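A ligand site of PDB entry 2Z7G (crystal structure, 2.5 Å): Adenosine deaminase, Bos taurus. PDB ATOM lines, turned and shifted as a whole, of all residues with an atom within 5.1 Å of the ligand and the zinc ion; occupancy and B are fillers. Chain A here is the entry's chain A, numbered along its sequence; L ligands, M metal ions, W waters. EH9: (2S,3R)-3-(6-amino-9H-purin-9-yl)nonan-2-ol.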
ATOM      1  N   HIS A  14     -15.305  -8.567 -22.659  1.00  0.00           N
ATOM      2  CA  HIS A  14     -16.465  -8.660 -23.533  1.00  0.00           C
ATOM      3  C   HIS A  14     -16.481  -9.831 -24.531  1.00  0.00           C
ATOM      4  O   HIS A  14     -16.052  -9.694 -25.678  1.00  0.00           O
ATOM      5  CB  HIS A  14     -16.662  -7.332 -24.287  1.00  0.00           C
ATOM      6  CG  HIS A  14     -18.004  -7.181 -24.903  1.00  0.00           C
ATOM      7  ND1 HIS A  14     -18.813  -6.083 -24.684  1.00  0.00           N
ATOM      8  CD2 HIS A  14     -18.713  -8.004 -25.731  1.00  0.00           C
ATOM      9  CE1 HIS A  14     -19.945  -6.224 -25.351  1.00  0.00           C
ATOM     10  NE2 HIS A  14     -19.914  -7.384 -25.998  1.00  0.00           N
ATOM     11  N   HIS A  16     -19.079 -13.355 -25.624  1.00  0.00           N
ATOM     12  CA  HIS A  16     -20.283 -14.197 -25.473  1.00  0.00           C
ATOM     13  C   HIS A  16     -19.991 -15.706 -25.480  1.00  0.00           C
ATOM     14  O   HIS A  16     -19.317 -16.194 -26.362  1.00  0.00           O
ATOM     15  CB  HIS A  16     -21.260 -13.888 -26.621  1.00  0.00           C
ATOM     16  CG  HIS A  16     -21.719 -12.482 -26.655  1.00  0.00           C
ATOM     17  ND1 HIS A  16     -22.887 -12.046 -26.059  1.00  0.00           N
ATOM     18  CD2 HIS A  16     -21.163 -11.363 -27.193  1.00  0.00           C
ATOM     19  CE1 HIS A  16     -23.032 -10.741 -26.202  1.00  0.00           C
ATOM     20  NE2 HIS A  16     -21.980 -10.306 -26.890  1.00  0.00           N
ATOM     21  N   ASP A  18     -22.152 -18.186 -25.975  1.00  0.00           N
ATOM     22  CA  ASP A  18     -22.860 -18.751 -27.123  1.00  0.00           C
ATOM     23  C   ASP A  18     -22.308 -18.297 -28.479  1.00  0.00           C
ATOM     24  O   ASP A  18     -22.854 -18.634 -29.519  1.00  0.00           O
ATOM     25  CB  ASP A  18     -24.366 -18.463 -27.024  1.00  0.00           C
ATOM     26  CG  ASP A  18     -24.685 -17.003 -26.716  1.00  0.00           C
ATOM     27  OD1 ASP A  18     -25.848 -16.713 -26.386  1.00  0.00           O
ATOM     28  OD2 ASP A  18     -23.784 -16.141 -26.806  1.00  0.00           O
ATOM     29  N   GLY A  19     -21.232 -17.519 -28.440  1.00  0.00           N
ATOM     30  CA  GLY A  19     -20.594 -17.055 -29.668  1.00  0.00           C
ATOM     31  C   GLY A  19     -19.148 -17.477 -29.618  1.00  0.00           C
ATOM     32  O   GLY A  19     -18.291 -16.958 -30.334  1.00  0.00           O
ATOM     33  N   LEU A  57     -29.134  -7.498 -39.767  1.00  0.00           N
ATOM     34  CA  LEU A  57     -29.399  -8.054 -38.452  1.00  0.00           C
ATOM     35  C   LEU A  57     -29.946  -9.478 -38.609  1.00  0.00           C
ATOM     36  O   LEU A  57     -29.457 -10.414 -37.994  1.00  0.00           O
ATOM     37  CB  LEU A  57     -30.419  -7.192 -37.701  1.00  0.00           C
ATOM     38  CG  LEU A  57     -30.849  -7.727 -36.328  1.00  0.00           C
ATOM     39  CD1 LEU A  57     -29.631  -7.969 -35.469  1.00  0.00           C
ATOM     40  CD2 LEU A  57     -31.777  -6.723 -35.651  1.00  0.00           C
ATOM     41  N   PHE A  60     -27.533 -12.063 -39.683  1.00  0.00           N
ATOM     42  CA  PHE A  60     -26.681 -12.271 -38.510  1.00  0.00           C
ATOM     43  C   PHE A  60     -27.335 -13.126 -37.428  1.00  0.00           C
ATOM     44  O   PHE A  60     -26.731 -14.046 -36.891  1.00  0.00           O
ATOM     45  CB  PHE A  60     -26.319 -10.920 -37.893  1.00  0.00           C
ATOM     46  CG  PHE A  60     -25.530 -11.046 -36.615  1.00  0.00           C
ATOM     47  CD1 PHE A  60     -24.199 -11.442 -36.646  1.00  0.00           C
ATOM     48  CD2 PHE A  60     -26.134 -10.809 -35.391  1.00  0.00           C
ATOM     49  CE1 PHE A  60     -23.494 -11.593 -35.471  1.00  0.00           C
ATOM     50  CE2 PHE A  60     -25.424 -10.957 -34.207  1.00  0.00           C
ATOM     51  CZ  PHE A  60     -24.102 -11.359 -34.256  1.00  0.00           C
ATOM     52  N   LEU A  61     -28.585 -12.779 -37.098  1.00  0.00           N
ATOM     53  CA  LEU A  61     -29.342 -13.489 -36.094  1.00  0.00           C
ATOM     54  C   LEU A  61     -29.463 -14.953 -36.511  1.00  0.00           C
ATOM     55  O   LEU A  61     -29.205 -15.869 -35.718  1.00  0.00           O
ATOM     56  CB  LEU A  61     -30.735 -12.876 -35.953  1.00  0.00           C
ATOM     57  CG  LEU A  61     -31.908 -13.808 -36.277  1.00  0.00           C
ATOM     58  CD1 LEU A  61     -32.059 -14.849 -35.159  1.00  0.00           C
ATOM     59  CD2 LEU A  61     -33.204 -13.002 -36.433  1.00  0.00           C
ATOM     60  N   PHE A  64     -27.398 -17.895 -35.302  1.00  0.00           N
ATOM     61  CA  PHE A  64     -27.677 -18.605 -34.057  1.00  0.00           C
ATOM     62  C   PHE A  64     -28.707 -19.722 -34.195  1.00  0.00           C
ATOM     63  O   PHE A  64     -28.563 -20.766 -33.550  1.00  0.00           O
ATOM     64  CB  PHE A  64     -28.096 -17.615 -32.967  1.00  0.00           C
ATOM     65  CG  PHE A  64     -27.035 -16.610 -32.615  1.00  0.00           C
ATOM     66  CD1 PHE A  64     -26.869 -15.454 -33.377  1.00  0.00           C
ATOM     67  CD2 PHE A  64     -26.173 -16.826 -31.546  1.00  0.00           C
ATOM     68  CE1 PHE A  64     -25.852 -14.550 -33.088  1.00  0.00           C
ATOM     69  CE2 PHE A  64     -25.152 -15.933 -31.244  1.00  0.00           C
ATOM     70  CZ  PHE A  64     -25.003 -14.779 -32.009  1.00  0.00           C
ATOM     71  N   ARG A 100     -20.016 -13.797 -20.932  1.00  0.00           N
ATOM     72  CA  ARG A 100     -21.445 -13.495 -20.815  1.00  0.00           C
ATOM     73  C   ARG A 100     -22.345 -14.318 -21.751  1.00  0.00           C
ATOM     74  O   ARG A 100     -21.895 -14.843 -22.771  1.00  0.00           O
ATOM     75  CB  ARG A 100     -21.692 -12.015 -21.081  1.00  0.00           C
ATOM     76  CG  ARG A 100     -21.358 -11.575 -22.495  1.00  0.00           C
ATOM     77  CD  ARG A 100     -21.511 -10.074 -22.650  1.00  0.00           C
ATOM     78  NE  ARG A 100     -20.451  -9.342 -21.974  1.00  0.00           N
ATOM     79  CZ  ARG A 100     -20.403  -8.020 -21.880  1.00  0.00           C
ATOM     80  NH1 ARG A 100     -19.398  -7.424 -21.263  1.00  0.00           N
ATOM     81  NH2 ARG A 100     -21.357  -7.278 -22.397  1.00  0.00           N
ATOM     82  N   TYR A 101     -23.617 -14.395 -21.384  1.00  0.00           N
ATOM     83  CA  TYR A 101     -24.592 -15.138 -22.151  1.00  0.00           C
ATOM     84  C   TYR A 101     -25.986 -14.999 -21.521  1.00  0.00           C
ATOM     85  O   TYR A 101     -26.126 -14.613 -20.370  1.00  0.00           O
ATOM     86  CB  TYR A 101     -24.194 -16.620 -22.169  1.00  0.00           C
ATOM     87  CG  TYR A 101     -24.329 -17.265 -20.815  1.00  0.00           C
ATOM     88  CD1 TYR A 101     -25.476 -17.994 -20.485  1.00  0.00           C
ATOM     89  CD2 TYR A 101     -23.369 -17.078 -19.835  1.00  0.00           C
ATOM     90  CE1 TYR A 101     -25.640 -18.523 -19.211  1.00  0.00           C
ATOM     91  CE2 TYR A 101     -23.535 -17.598 -18.552  1.00  0.00           C
ATOM     92  CZ  TYR A 101     -24.672 -18.313 -18.254  1.00  0.00           C
ATOM     93  OH  TYR A 101     -24.865 -18.816 -16.986  1.00  0.00           O
ATOM     94  N   SER A 102     -27.002 -15.322 -22.309  1.00  0.00           N
ATOM     95  CA  SER A 102     -28.381 -15.248 -21.848  1.00  0.00           C
ATOM     96  C   SER A 102     -28.784 -16.650 -21.428  1.00  0.00           C
ATOM     97  O   SER A 102     -28.902 -17.551 -22.259  1.00  0.00           O
ATOM     98  CB  SER A 102     -29.301 -14.781 -22.991  1.00  0.00           C
ATOM     99  OG  SER A 102     -30.658 -14.895 -22.619  1.00  0.00           O
ATOM    100  N   LEU A 105     -31.654 -18.240 -23.292  1.00  0.00           N
ATOM    101  CA  LEU A 105     -31.380 -18.691 -24.643  1.00  0.00           C
ATOM    102  C   LEU A 105     -30.814 -20.109 -24.756  1.00  0.00           C
ATOM    103  O   LEU A 105     -30.643 -20.635 -25.855  1.00  0.00           O
ATOM    104  CB  LEU A 105     -30.462 -17.690 -25.353  1.00  0.00           C
ATOM    105  CG  LEU A 105     -31.135 -16.318 -25.485  1.00  0.00           C
ATOM    106  CD1 LEU A 105     -30.292 -15.386 -26.322  1.00  0.00           C
ATOM    107  CD2 LEU A 105     -32.494 -16.503 -26.115  1.00  0.00           C
ATOM    108  N   TRP A 116     -35.359 -20.631 -30.240  1.00  0.00           N
ATOM    109  CA  TRP A 116     -34.922 -21.513 -31.314  1.00  0.00           C
ATOM    110  C   TRP A 116     -35.914 -22.594 -31.776  1.00  0.00           C
ATOM    111  O   TRP A 116     -35.496 -23.655 -32.240  1.00  0.00           O
ATOM    112  CB  TRP A 116     -33.614 -22.186 -30.886  1.00  0.00           C
ATOM    113  CG  TRP A 116     -32.716 -21.273 -30.091  1.00  0.00           C
ATOM    114  CD1 TRP A 116     -32.356 -21.420 -28.784  1.00  0.00           C
ATOM    115  CD2 TRP A 116     -32.124 -20.049 -30.530  1.00  0.00           C
ATOM    116  NE1 TRP A 116     -31.568 -20.369 -28.380  1.00  0.00           N
ATOM    117  CE2 TRP A 116     -31.409 -19.514 -29.433  1.00  0.00           C
ATOM    118  CE3 TRP A 116     -32.116 -19.355 -31.738  1.00  0.00           C
ATOM    119  CZ2 TRP A 116     -30.702 -18.315 -29.517  1.00  0.00           C
ATOM    120  CZ3 TRP A 116     -31.409 -18.170 -31.819  1.00  0.00           C
ATOM    121  CH2 TRP A 116     -30.711 -17.663 -30.717  1.00  0.00           C
ATOM    122  N   CYS A 152     -26.921 -11.927 -19.486  1.00  0.00           N
ATOM    123  CA  CYS A 152     -27.496 -10.899 -20.330  1.00  0.00           C
ATOM    124  C   CYS A 152     -29.022 -10.835 -20.313  1.00  0.00           C
ATOM    125  O   CYS A 152     -29.695 -11.848 -20.176  1.00  0.00           O
ATOM    126  CB  CYS A 152     -27.071 -11.100 -21.769  1.00  0.00           C
ATOM    127  SG  CYS A 152     -25.277 -11.213 -22.017  1.00  0.00           S
ATOM    128  N   MET A 154     -32.236  -9.343 -22.563  1.00  0.00           N
ATOM    129  CA  MET A 154     -32.401  -9.118 -23.993  1.00  0.00           C
ATOM    130  C   MET A 154     -33.309  -7.904 -24.244  1.00  0.00           C
ATOM    131  O   MET A 154     -34.448  -7.848 -23.761  1.00  0.00           O
ATOM    132  CB  MET A 154     -32.964 -10.360 -24.678  1.00  0.00           C
ATOM    133  CG  MET A 154     -32.121 -11.625 -24.496  1.00  0.00           C
ATOM    134  SD  MET A 154     -30.395 -11.449 -25.054  1.00  0.00           S
ATOM    135  CE  MET A 154     -30.644 -11.110 -26.789  1.00  0.00           C
ATOM    136  N   ALA A 182     -28.138  -6.965 -23.989  1.00  0.00           N
ATOM    137  CA  ALA A 182     -27.657  -7.178 -25.347  1.00  0.00           C
ATOM    138  C   ALA A 182     -28.877  -7.226 -26.264  1.00  0.00           C
ATOM    139  O   ALA A 182     -29.997  -7.165 -25.791  1.00  0.00           O
ATOM    140  CB  ALA A 182     -26.883  -8.480 -25.430  1.00  0.00           C
ATOM    141  N   GLY A 183     -28.643  -7.328 -27.580  1.00  0.00           N
ATOM    142  CA  GLY A 183     -29.766  -7.356 -28.512  1.00  0.00           C
ATOM    143  C   GLY A 183     -29.918  -6.112 -29.375  1.00  0.00           C
ATOM    144  O   GLY A 183     -29.168  -5.137 -29.227  1.00  0.00           O
ATOM    145  N   HIS A 213     -24.711  -3.126 -23.571  1.00  0.00           N
ATOM    146  CA  HIS A 213     -24.266  -3.018 -24.966  1.00  0.00           C
ATOM    147  C   HIS A 213     -24.959  -1.749 -25.490  1.00  0.00           C
ATOM    148  O   HIS A 213     -26.165  -1.744 -25.690  1.00  0.00           O
ATOM    149  CB  HIS A 213     -24.777  -4.199 -25.819  1.00  0.00           C
ATOM    150  CG  HIS A 213     -23.933  -5.442 -25.735  1.00  0.00           C
ATOM    151  ND1 HIS A 213     -23.977  -6.303 -24.663  1.00  0.00           N
ATOM    152  CD2 HIS A 213     -23.091  -5.992 -26.639  1.00  0.00           C
ATOM    153  CE1 HIS A 213     -23.193  -7.341 -24.901  1.00  0.00           C
ATOM    154  NE2 HIS A 213     -22.646  -7.176 -26.086  1.00  0.00           N
ATOM    155  N   GLU A 216     -22.950   0.634 -30.136  1.00  0.00           N
ATOM    156  CA  GLU A 216     -22.399  -0.202 -31.185  1.00  0.00           C
ATOM    157  C   GLU A 216     -23.019   0.188 -32.530  1.00  0.00           C
ATOM    158  O   GLU A 216     -22.318   0.391 -33.523  1.00  0.00           O
ATOM    159  CB  GLU A 216     -22.664  -1.698 -30.889  1.00  0.00           C
ATOM    160  CG  GLU A 216     -22.309  -2.633 -32.036  1.00  0.00           C
ATOM    161  CD  GLU A 216     -22.450  -4.118 -31.685  1.00  0.00           C
ATOM    162  OE1 GLU A 216     -23.486  -4.516 -31.097  1.00  0.00           O
ATOM    163  OE2 GLU A 216     -21.546  -4.892 -32.035  1.00  0.00           O
ATOM    164  N   HIS A 237     -18.935  -1.742 -26.277  1.00  0.00           N
ATOM    165  CA  HIS A 237     -18.756  -1.013 -27.527  1.00  0.00           C
ATOM    166  C   HIS A 237     -18.747   0.505 -27.316  1.00  0.00           C
ATOM    167  O   HIS A 237     -17.680   1.109 -27.219  1.00  0.00           O
ATOM    168  CB  HIS A 237     -19.871  -1.376 -28.520  1.00  0.00           C
ATOM    169  CG  HIS A 237     -19.895  -2.812 -28.898  1.00  0.00           C
ATOM    170  ND1 HIS A 237     -18.859  -3.426 -29.561  1.00  0.00           N
ATOM    171  CD2 HIS A 237     -20.844  -3.764 -28.735  1.00  0.00           C
ATOM    172  CE1 HIS A 237     -19.169  -4.688 -29.784  1.00  0.00           C
ATOM    173  NE2 HIS A 237     -20.376  -4.919 -29.296  1.00  0.00           N
ATOM    174  N   ASP A 294     -15.524 -10.694 -28.534  1.00  0.00           N
ATOM    175  CA  ASP A 294     -16.985 -10.678 -28.679  1.00  0.00           C
ATOM    176  C   ASP A 294     -17.559 -12.054 -29.045  1.00  0.00           C
ATOM    177  O   ASP A 294     -18.249 -12.674 -28.235  1.00  0.00           O
ATOM    178  CB  ASP A 294     -17.371  -9.623 -29.742  1.00  0.00           C
ATOM    179  CG  ASP A 294     -18.769  -9.062 -29.526  1.00  0.00           C
ATOM    180  OD1 ASP A 294     -19.438  -9.414 -28.513  1.00  0.00           O
ATOM    181  OD2 ASP A 294     -19.205  -8.258 -30.387  1.00  0.00           O
ATOM    182  N   ASP A 295     -17.258 -12.535 -30.250  1.00  0.00           N
ATOM    183  CA  ASP A 295     -17.749 -13.841 -30.709  1.00  0.00           C
ATOM    184  C   ASP A 295     -16.724 -14.495 -31.628  1.00  0.00           C
ATOM    185  O   ASP A 295     -16.794 -14.353 -32.848  1.00  0.00           O
ATOM    186  CB  ASP A 295     -19.061 -13.704 -31.471  1.00  0.00           C
ATOM    187  CG  ASP A 295     -20.115 -12.956 -30.681  1.00  0.00           C
ATOM    188  OD1 ASP A 295     -21.043 -13.604 -30.121  1.00  0.00           O
ATOM    189  OD2 ASP A 295     -20.009 -11.715 -30.610  1.00  0.00           O
HETATM  190  C1  EH9 L   1     -24.089 -10.014 -30.211  1.00  0.00           C
HETATM  191  C2  EH9 L   1     -24.124 -11.251 -29.632  1.00  0.00           C
HETATM  192  C3  EH9 L   1     -25.277 -11.654 -28.955  1.00  0.00           C
HETATM  193  C5  EH9 L   1     -26.327  -9.674 -29.424  1.00  0.00           C
HETATM  194  C14 EH9 L   1     -23.783 -13.252 -28.917  1.00  0.00           C
HETATM  195  N4  EH9 L   1     -26.401 -10.880 -28.836  1.00  0.00           N
HETATM  196  N6  EH9 L   1     -25.226  -9.238 -30.087  1.00  0.00           N
HETATM  197  N13 EH9 L   1     -25.023 -12.918 -28.485  1.00  0.00           N
HETATM  198  N15 EH9 L   1     -23.226 -12.214 -29.579  1.00  0.00           N
HETATM  199  C20 EH9 L   1     -25.791 -13.901 -27.700  1.00  0.00           C
HETATM  200  C21 EH9 L   1     -26.963 -14.579 -28.456  1.00  0.00           C
HETATM  201  N24 EH9 L   1     -23.026  -9.530 -30.884  1.00  0.00           N
HETATM  202  C26 EH9 L   1     -28.008 -13.608 -28.991  1.00  0.00           C
HETATM  203  C28 EH9 L   1     -29.161 -14.143 -29.812  1.00  0.00           C
HETATM  204  C30 EH9 L   1     -29.877 -12.913 -30.416  1.00  0.00           C
HETATM  205  C31 EH9 L   1     -28.892 -11.888 -31.027  1.00  0.00           C
HETATM  206  C34 EH9 L   1     -29.300 -11.348 -32.400  1.00  0.00           C
HETATM  207  C36 EH9 L   1     -26.004 -13.554 -26.231  1.00  0.00           C
HETATM  208  O38 EH9 L   1     -24.772 -13.619 -25.568  1.00  0.00           O
HETATM  209  C40 EH9 L   1     -26.939 -12.408 -25.845  1.00  0.00           C
HETATM  210 ZN    ZN M   1     -21.253  -8.372 -27.482  1.00  0.00          ZN
HETATM  211  O   HOH W   1     -26.318  -6.678 -28.518  1.00  0.00           O
HETATM  212  O   HOH W   2     -21.313  -7.555 -29.382  1.00  0.00           O
HETATM  213  O   HOH W   3     -21.750  -7.339 -32.920  1.00  0.00           O
HETATM  214  O   HOH W   4     -23.820  -6.692 -29.888  1.00  0.00           O
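O of Tyr 101 is in hydrogen-bond range of N of Cys 152 (2.9 Å). A ring nitrogen (NE2) of His 237 lies within hydrogen-bond range of the side-chain carboxylate (OE2) of Glu 216 (3.0 Å). The indole nitrogen (NE1) of Trp 116 is in hydrogen-bond range of the backbone carbonyl oxygen (O) of Leu 105 (2.7 Å).
The zinc ion is bound by water W2. A ring nitrogen (NE2) of His 16 binds the zinc ion, at 2.1 Å. The zinc ion is bound by NE2 of His 14 (2.2 Å). NE2 of His 213 binds the zinc ion (2.3 Å). The zinc ion is bound by OD1 of Asp 294 (2.3 Å). The zinc ion has five donor atoms within binding distance.
Water W2 lies within hydrogen-bond range of the side-chain carboxylate of Asp 294, a ring nitrogen (NE2) of His 237 and a nitrogen (N24) of the ligand. Water W4 bridges the side-chain carboxylate of Glu 216 (2.5 Å) and a nitrogen (N6) of the ligand (2.9 Å). Water W1 lies within hydrogen-bond range of N of Gly 183 (2.6 Å) and N6 of the ligand (3.2 Å). Water W3 bridges OE2 of Glu 216 and N24 of the ligand.
Residues that only touch the ligand: Phe 64, Met 154, Tyr 101, Gly 183, Leu 105, Ala 182, Trp 116 and Phe 60. The nearest printed residue that does not touch the ligand is Asp 294 (4.1 Å).
His 237 touches the zinc ion (NE2 to ZN, 3.998 Å). Of the 22 residues printed, 5 come within 4 Å of the zinc ion.
OD1 of Asp 295 sits at hydrogen-bond distance from N15 of the ligand (2.6 Å). A ring nitrogen (ND1) of His 16 sits at hydrogen-bond distance from an oxygen (O38) of the ligand, 2.5 Å away. The side-chain carboxylate (OD2) of Asp 18 sits at hydrogen-bond distance from an oxygen (O38) of the ligand (3.0 Å).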
